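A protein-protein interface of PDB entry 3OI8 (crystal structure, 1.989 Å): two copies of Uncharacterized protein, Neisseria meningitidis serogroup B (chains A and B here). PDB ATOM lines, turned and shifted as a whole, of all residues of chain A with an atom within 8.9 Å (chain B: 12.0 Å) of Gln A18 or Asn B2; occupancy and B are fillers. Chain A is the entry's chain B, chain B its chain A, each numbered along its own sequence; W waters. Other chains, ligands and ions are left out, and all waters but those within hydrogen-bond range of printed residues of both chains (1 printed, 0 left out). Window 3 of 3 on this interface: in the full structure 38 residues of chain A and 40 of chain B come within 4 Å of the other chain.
The backbone NH of Ala B3 sits close to the side-chain amide oxygen of Gln A18 (3.3 Å).
Leu A11 touches its own counterpart, Leu B11. Positions printed for both chains: 10 and 11.
Gln A18 touches just these residues of chain B: Asn B2 and Ala B3. Asn B2 touches just one residue of chain A: Gln A18. No residue of chain B comes within 4 Å of Gln A14. No residue of chain B comes within 4 Å of His A16. Glu A17 touches none of the printed residues of chain B. No residue of chain B comes within 4 Å of Glu A19. No residue of chain A comes within 4 Å of Ser B1. Of chain A, only Gln A18 (3.1 Å) and Val A20 (3.8 Å) come within 4 Å of Ala B3. Printed residues of chain B within 4 Å of Val A20: Ala B3, Ser B4 and Ala B5. Printed residues of chain A within 4 Å of Ser B4: Val A20 (3.9 Å). Asp A22 touches none of the printed residues of chain B. Leu B9 touches none of the printed residues of chain A. The nearest residue of chain B that does not touch Gln A18 is Ser B1 (4.3 Å). The nearest residue of chain A that does not touch Asn B2 is Val A20 (6.3 Å).
The backbone NH (N) of Glu B6 lies close to the side-chain hydroxyl (OG) of Ser B4, 3.4 Å away. N of Ser B4 is in hydrogen-bond range of OD2 of Asp B7. The backbone carbonyl oxygen (O) of Gln A14 sits close to the side-chain amide nitrogen (NE2) of Gln A18 (3.3 Å). The backbone carbonyl oxygen (O) of Ala A15 is in hydrogen-bond range of the backbone NH (N) of Val A20, at 2.8 Å.
Among the printed residues, pairs that only touch across the chains: Leu A11 with Leu B11 (3.3 Å), Leu A12 with Val B8 (3.8 Å), Ala A15 with Val B8 (3.6 Å), Gln A18 with Asn B2 (3.3 Å), Val A20 with Ala B3 (3.8 Å), Val A20 with Ser B4 (3.9 Å) and Val A20 with Ala B5 (3.7 Å).
Water W1 bridges the side-chain hydroxyl of Ser B36 (2.9 Å) and the backbone carbonyl oxygen of Val A20 (3.2 Å).
Printed residues of chain B that touch a printed residue of chain A: Asn B2, Ala B3, Ser B4, Ala B5, Val B8 and Leu B11. Hydrophobic or aromatic side chains of chain B that line the printed part of chain A: Ala B3, Val B8 and Leu B11. Of the 13 printed residues of chain A, 5 touch a printed residue of chain B. Among the printed residues, 8 pairs touch across the chains. Among the printed residues, no Asp or Glu carboxylate lies within 4 Å of a Lys or Arg side-chain nitrogen of the other chain.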
ATOM      1  N   ASN A  10      25.112  21.128   6.334  1.00  0.00           N
ATOM      2  CA  ASN A  10      23.911  20.794   7.083  1.00  0.00           C
ATOM      3  C   ASN A  10      23.692  21.682   8.306  1.00  0.00           C
ATOM      4  O   ASN A  10      22.564  21.815   8.789  1.00  0.00           O
ATOM      5  CB  ASN A  10      23.821  19.301   7.423  1.00  0.00           C
ATOM      6  CG  ASN A  10      25.132  18.729   7.893  1.00  0.00           C
ATOM      7  OD1 ASN A  10      25.379  18.617   9.095  1.00  0.00           O
ATOM      8  ND2 ASN A  10      25.981  18.350   6.944  1.00  0.00           N
ATOM      9  N   LEU A  11      24.757  22.306   8.800  1.00  0.00           N
ATOM     10  CA  LEU A  11      24.593  23.268   9.891  1.00  0.00           C
ATOM     11  C   LEU A  11      24.024  24.594   9.378  1.00  0.00           C
ATOM     12  O   LEU A  11      23.296  25.293  10.082  1.00  0.00           O
ATOM     13  CB  LEU A  11      25.904  23.481  10.638  1.00  0.00           C
ATOM     14  CG  LEU A  11      26.180  22.348  11.627  1.00  0.00           C
ATOM     15  CD1 LEU A  11      27.642  22.338  12.040  1.00  0.00           C
ATOM     16  CD2 LEU A  11      25.246  22.433  12.844  1.00  0.00           C
ATOM     17  N   LEU A  12      24.356  24.925   8.144  1.00  0.00           N
ATOM     18  CA  LEU A  12      23.749  26.078   7.492  1.00  0.00           C
ATOM     19  C   LEU A  12      22.251  25.866   7.312  1.00  0.00           C
ATOM     20  O   LEU A  12      21.463  26.791   7.496  1.00  0.00           O
ATOM     21  CB  LEU A  12      24.410  26.327   6.151  1.00  0.00           C
ATOM     22  CG  LEU A  12      25.787  26.985   6.228  1.00  0.00           C
ATOM     23  CD1 LEU A  12      26.290  27.310   4.832  1.00  0.00           C
ATOM     24  CD2 LEU A  12      25.743  28.240   7.099  1.00  0.00           C
ATOM     25  N   ARG A  13      21.863  24.640   6.968  1.00  0.00           N
ATOM     26  CA  ARG A  13      20.451  24.293   6.821  1.00  0.00           C
ATOM     27  C   ARG A  13      19.727  24.373   8.156  1.00  0.00           C
ATOM     28  O   ARG A  13      18.575  24.798   8.228  1.00  0.00           O
ATOM     29  CB  ARG A  13      20.301  22.892   6.242  1.00  0.00           C
ATOM     30  CG  ARG A  13      21.203  22.625   5.058  1.00  0.00           C
ATOM     31  CD  ARG A  13      21.138  21.168   4.655  1.00  0.00           C
ATOM     32  NE  ARG A  13      22.326  20.763   3.914  1.00  0.00           N
ATOM     33  CZ  ARG A  13      22.500  20.969   2.614  1.00  0.00           C
ATOM     34  NH1 ARG A  13      21.557  21.578   1.909  1.00  0.00           N
ATOM     35  NH2 ARG A  13      23.615  20.568   2.020  1.00  0.00           N
ATOM     36  N   GLN A  14      20.408  23.959   9.217  1.00  0.00           N
ATOM     37  CA  GLN A  14      19.831  24.026  10.549  1.00  0.00           C
ATOM     38  C   GLN A  14      19.576  25.469  10.955  1.00  0.00           C
ATOM     39  O   GLN A  14      18.578  25.767  11.618  1.00  0.00           O
ATOM     40  CB  GLN A  14      20.743  23.353  11.580  1.00  0.00           C
ATOM     41  CG  GLN A  14      20.803  21.841  11.492  1.00  0.00           C
ATOM     42  CD  GLN A  14      21.256  21.206  12.807  1.00  0.00           C
ATOM     43  OE1 GLN A  14      21.784  21.884  13.690  1.00  0.00           O
ATOM     44  NE2 GLN A  14      21.041  19.902  12.940  1.00  0.00           N
ATOM     45  N   ALA A  15      20.481  26.367  10.570  1.00  0.00           N
ATOM     46  CA  ALA A  15      20.351  27.762  10.967  1.00  0.00           C
ATOM     47  C   ALA A  15      19.148  28.356  10.250  1.00  0.00           C
ATOM     48  O   ALA A  15      18.545  29.325  10.710  1.00  0.00           O
ATOM     49  CB  ALA A  15      21.623  28.536  10.644  1.00  0.00           C
ATOM     50  N   HIS A  16      18.805  27.748   9.122  1.00  0.00           N
ATOM     51  CA  HIS A  16      17.684  28.184   8.301  1.00  0.00           C
ATOM     52  C   HIS A  16      16.374  27.765   8.955  1.00  0.00           C
ATOM     53  O   HIS A  16      15.441  28.565   9.085  1.00  0.00           O
ATOM     54  CB  HIS A  16      17.807  27.588   6.896  1.00  0.00           C
ATOM     55  CG  HIS A  16      16.589  27.772   6.048  1.00  0.00           C
ATOM     56  ND1 HIS A  16      15.855  28.938   6.038  1.00  0.00           N
ATOM     57  CD2 HIS A  16      15.986  26.941   5.164  1.00  0.00           C
ATOM     58  CE1 HIS A  16      14.843  28.813   5.198  1.00  0.00           C
ATOM     59  NE2 HIS A  16      14.902  27.612   4.652  1.00  0.00           N
ATOM     60  N   GLU A  17      16.322  26.510   9.387  1.00  0.00           N
ATOM     61  CA  GLU A  17      15.145  25.981  10.067  1.00  0.00           C
ATOM     62  C   GLU A  17      14.950  26.653  11.422  1.00  0.00           C
ATOM     63  O   GLU A  17      13.904  26.505  12.055  1.00  0.00           O
ATOM     64  CB  GLU A  17      15.265  24.467  10.232  1.00  0.00           C
ATOM     65  CG  GLU A  17      15.547  23.727   8.934  1.00  0.00           C
ATOM     66  CD  GLU A  17      15.673  22.226   9.129  1.00  0.00           C
ATOM     67  OE1 GLU A  17      15.151  21.705  10.139  1.00  0.00           O
ATOM     68  OE2 GLU A  17      16.294  21.566   8.265  1.00  0.00           O
ATOM     69  N   GLN A  18      15.960  27.394  11.864  1.00  0.00           N
ATOM     70  CA  GLN A  18      15.880  28.124  13.123  1.00  0.00           C
ATOM     71  C   GLN A  18      15.602  29.608  12.893  1.00  0.00           C
ATOM     72  O   GLN A  18      15.635  30.402  13.833  1.00  0.00           O
ATOM     73  CB  GLN A  18      17.165  27.942  13.938  1.00  0.00           C
ATOM     74  CG  GLN A  18      17.448  26.501  14.350  1.00  0.00           C
ATOM     75  CD  GLN A  18      18.776  26.349  15.069  1.00  0.00           C
ATOM     76  OE1 GLN A  18      19.130  27.167  15.917  1.00  0.00           O
ATOM     77  NE2 GLN A  18      19.517  25.298  14.734  1.00  0.00           N
ATOM     78  N   GLU A  19      15.340  29.973  11.639  1.00  0.00           N
ATOM     79  CA  GLU A  19      14.949  31.338  11.278  1.00  0.00           C
ATOM     80  C   GLU A  19      16.103  32.336  11.231  1.00  0.00           C
ATOM     81  O   GLU A  19      15.878  33.545  11.299  1.00  0.00           O
ATOM     82  CB  GLU A  19      13.865  31.868  12.225  1.00  0.00           C
ATOM     83  CG  GLU A  19      12.474  31.290  12.003  1.00  0.00           C
ATOM     84  CD  GLU A  19      11.474  31.767  13.045  1.00  0.00           C
ATOM     85  OE1 GLU A  19      11.807  31.738  14.247  1.00  0.00           O
ATOM     86  OE2 GLU A  19      10.353  32.169  12.662  1.00  0.00           O
ATOM     87  N   VAL A  20      17.333  31.846  11.115  1.00  0.00           N
ATOM     88  CA  VAL A  20      18.487  32.741  11.069  1.00  0.00           C
ATOM     89  C   VAL A  20      18.530  33.474   9.726  1.00  0.00           C
ATOM     90  O   VAL A  20      18.792  34.682   9.663  1.00  0.00           O
ATOM     91  CB  VAL A  20      19.821  31.985  11.333  1.00  0.00           C
ATOM     92  CG1 VAL A  20      20.996  32.936  11.213  1.00  0.00           C
ATOM     93  CG2 VAL A  20      19.807  31.327  12.710  1.00  0.00           C
ATOM     94  N   PHE A  21      18.270  32.731   8.652  1.00  0.00           N
ATOM     95  CA  PHE A  21      18.103  33.309   7.330  1.00  0.00           C
ATOM     96  C   PHE A  21      17.118  32.460   6.532  1.00  0.00           C
ATOM     97  O   PHE A  21      16.834  31.318   6.889  1.00  0.00           O
ATOM     98  CB  PHE A  21      19.451  33.411   6.595  1.00  0.00           C
ATOM     99  CG  PHE A  21      20.278  32.149   6.667  1.00  0.00           C
ATOM    100  CD1 PHE A  21      21.304  32.028   7.592  1.00  0.00           C
ATOM    101  CD2 PHE A  21      20.025  31.086   5.812  1.00  0.00           C
ATOM    102  CE1 PHE A  21      22.065  30.859   7.665  1.00  0.00           C
ATOM    103  CE2 PHE A  21      20.782  29.922   5.871  1.00  0.00           C
ATOM    104  CZ  PHE A  21      21.804  29.808   6.810  1.00  0.00           C
ATOM    105  N   ASP A  22      16.617  33.022   5.440  1.00  0.00           N
ATOM    106  CA  ASP A  22      15.585  32.382   4.628  1.00  0.00           C
ATOM    107  C   ASP A  22      16.153  31.490   3.524  1.00  0.00           C
ATOM    108  O   ASP A  22      17.360  31.494   3.258  1.00  0.00           O
ATOM    109  CB  ASP A  22      14.666  33.450   4.009  1.00  0.00           C
ATOM    110  CG  ASP A  22      15.411  34.406   3.083  1.00  0.00           C
ATOM    111  OD1 ASP A  22      16.443  34.006   2.502  1.00  0.00           O
ATOM    112  OD2 ASP A  22      14.961  35.562   2.934  1.00  0.00           O
ATOM    113  N   SER B   1      17.073  24.053  18.957  1.00  0.00           N
ATOM    114  CA  SER B   1      17.409  24.925  20.077  1.00  0.00           C
ATOM    115  C   SER B   1      17.195  26.402  19.736  1.00  0.00           C
ATOM    116  O   SER B   1      16.060  26.882  19.711  1.00  0.00           O
ATOM    117  CB  SER B   1      18.843  24.668  20.554  1.00  0.00           C
ATOM    118  OG  SER B   1      19.679  24.248  19.488  1.00  0.00           O
ATOM    119  N   ASN B   2      18.284  27.121  19.480  1.00  0.00           N
ATOM    120  CA  ASN B   2      18.194  28.531  19.105  1.00  0.00           C
ATOM    121  C   ASN B   2      19.534  29.045  18.591  1.00  0.00           C
ATOM    122  O   ASN B   2      20.592  28.628  19.072  1.00  0.00           O
ATOM    123  CB  ASN B   2      17.707  29.378  20.283  1.00  0.00           C
ATOM    124  CG  ASN B   2      16.680  30.420  19.872  1.00  0.00           C
ATOM    125  OD1 ASN B   2      16.885  31.170  18.916  1.00  0.00           O
ATOM    126  ND2 ASN B   2      15.570  30.474  20.602  1.00  0.00           N
ATOM    127  N   ALA B   3      19.490  29.943  17.611  1.00  0.00           N
ATOM    128  CA  ALA B   3      20.714  30.414  16.971  1.00  0.00           C
ATOM    129  C   ALA B   3      20.643  31.867  16.518  1.00  0.00           C
ATOM    130  O   ALA B   3      19.580  32.492  16.527  1.00  0.00           O
ATOM    131  CB  ALA B   3      21.091  29.511  15.803  1.00  0.00           C
ATOM    132  N   SER B   4      21.800  32.384  16.122  1.00  0.00           N
ATOM    133  CA  SER B   4      21.954  33.763  15.692  1.00  0.00           C
ATOM    134  C   SER B   4      22.887  33.755  14.496  1.00  0.00           C
ATOM    135  O   SER B   4      23.571  32.765  14.262  1.00  0.00           O
ATOM    136  CB  SER B   4      22.580  34.584  16.814  1.00  0.00           C
ATOM    137  OG  SER B   4      22.694  35.947  16.453  1.00  0.00           O
ATOM    138  N   ALA B   5      22.928  34.847  13.742  1.00  0.00           N
ATOM    139  CA  ALA B   5      23.909  34.947  12.673  1.00  0.00           C
ATOM    140  C   ALA B   5      25.303  34.802  13.283  1.00  0.00           C
ATOM    141  O   ALA B   5      26.210  34.258  12.664  1.00  0.00           O
ATOM    142  CB  ALA B   5      23.772  36.267  11.938  1.00  0.00           C
ATOM    143  N   GLU B   6      25.457  35.276  14.515  1.00  0.00           N
ATOM    144  CA  GLU B   6      26.726  35.167  15.215  1.00  0.00           C
ATOM    145  C   GLU B   6      27.197  33.722  15.308  1.00  0.00           C
ATOM    146  O   GLU B   6      28.387  33.445  15.152  1.00  0.00           O
ATOM    147  CB  GLU B   6      26.617  35.757  16.619  1.00  0.00           C
ATOM    148  CG  GLU B   6      27.478  36.980  16.836  1.00  0.00           C
ATOM    149  CD  GLU B   6      27.510  37.412  18.290  1.00  0.00           C
ATOM    150  OE1 GLU B   6      27.707  36.541  19.171  1.00  0.00           O
ATOM    151  OE2 GLU B   6      27.343  38.624  18.551  1.00  0.00           O
ATOM    152  N   ASP B   7      26.275  32.799  15.572  1.00  0.00           N
ATOM    153  CA  ASP B   7      26.654  31.393  15.697  1.00  0.00           C
ATOM    154  C   ASP B   7      27.105  30.862  14.339  1.00  0.00           C
ATOM    155  O   ASP B   7      28.056  30.086  14.251  1.00  0.00           O
ATOM    156  CB  ASP B   7      25.506  30.555  16.277  1.00  0.00           C
ATOM    157  CG  ASP B   7      25.045  31.062  17.643  1.00  0.00           C
ATOM    158  OD1 ASP B   7      25.873  31.096  18.581  1.00  0.00           O
ATOM    159  OD2 ASP B   7      23.857  31.447  17.770  1.00  0.00           O
ATOM    160  N   VAL B   8      26.436  31.309  13.281  1.00  0.00           N
ATOM    161  CA  VAL B   8      26.792  30.902  11.922  1.00  0.00           C
ATOM    162  C   VAL B   8      28.175  31.452  11.557  1.00  0.00           C
ATOM    163  O   VAL B   8      29.020  30.730  11.031  1.00  0.00           O
ATOM    164  CB  VAL B   8      25.741  31.421  10.890  1.00  0.00           C
ATOM    165  CG1 VAL B   8      26.210  31.144   9.476  1.00  0.00           C
ATOM    166  CG2 VAL B   8      24.381  30.778  11.140  1.00  0.00           C
ATOM    167  N   LEU B   9      28.397  32.732  11.857  1.00  0.00           N
ATOM    168  CA  LEU B   9      29.707  33.355  11.680  1.00  0.00           C
ATOM    169  C   LEU B   9      30.820  32.579  12.388  1.00  0.00           C
ATOM    170  O   LEU B   9      31.852  32.283  11.783  1.00  0.00           O
ATOM    171  CB  LEU B   9      29.688  34.810  12.162  1.00  0.00           C
ATOM    172  CG  LEU B   9      29.358  35.871  11.115  1.00  0.00           C
ATOM    173  CD1 LEU B   9      29.275  37.262  11.739  1.00  0.00           C
ATOM    174  CD2 LEU B   9      30.398  35.845  10.001  1.00  0.00           C
ATOM    175  N   ASN B  10      30.622  32.256  13.666  1.00  0.00           N
ATOM    176  CA  ASN B  10      31.597  31.433  14.397  1.00  0.00           C
ATOM    177  C   ASN B  10      31.847  30.118  13.679  1.00  0.00           C
ATOM    178  O   ASN B  10      32.992  29.687  13.501  1.00  0.00           O
ATOM    179  CB  ASN B  10      31.120  31.135  15.833  1.00  0.00           C
ATOM    180  CG  ASN B  10      31.137  32.355  16.716  1.00  0.00           C
ATOM    181  OD1 ASN B  10      31.651  33.410  16.333  1.00  0.00           O
ATOM    182  ND2 ASN B  10      30.567  32.227  17.914  1.00  0.00           N
ATOM    183  N   LEU B  11      30.756  29.471  13.292  1.00  0.00           N
ATOM    184  CA  LEU B  11      30.807  28.208  12.568  1.00  0.00           C
ATOM    185  C   LEU B  11      31.682  28.340  11.313  1.00  0.00           C
ATOM    186  O   LEU B  11      32.556  27.520  11.058  1.00  0.00           O
ATOM    187  CB  LEU B  11      29.387  27.829  12.159  1.00  0.00           C
ATOM    188  CG  LEU B  11      29.178  26.548  11.364  1.00  0.00           C
ATOM    189  CD1 LEU B  11      28.880  25.432  12.339  1.00  0.00           C
ATOM    190  CD2 LEU B  11      28.035  26.722  10.365  1.00  0.00           C
ATOM    191  N   LEU B  33      25.806  36.592   4.107  1.00  0.00           N
ATOM    192  CA  LEU B  33      25.119  36.639   5.383  1.00  0.00           C
ATOM    193  C   LEU B  33      24.636  38.036   5.728  1.00  0.00           C
ATOM    194  O   LEU B  33      23.515  38.206   6.206  1.00  0.00           O
ATOM    195  CB  LEU B  33      26.047  36.152   6.484  1.00  0.00           C
ATOM    196  CG  LEU B  33      25.739  34.733   6.940  1.00  0.00           C
ATOM    197  CD1 LEU B  33      26.746  34.310   7.995  1.00  0.00           C
ATOM    198  CD2 LEU B  33      24.331  34.682   7.481  1.00  0.00           C
ATOM    199  N   SER B  36      21.733  39.265   3.572  1.00  0.00           N
ATOM    200  CA  SER B  36      20.445  38.646   3.886  1.00  0.00           C
ATOM    201  C   SER B  36      19.644  39.482   4.874  1.00  0.00           C
ATOM    202  O   SER B  36      18.450  39.257   5.062  1.00  0.00           O
ATOM    203  CB  SER B  36      20.663  37.251   4.477  1.00  0.00           C
ATOM    204  OG  SER B  36      21.063  37.344   5.837  1.00  0.00           O
HETATM  205  O   HOH W   1      18.923  37.158   7.714  1.00  0.00           O
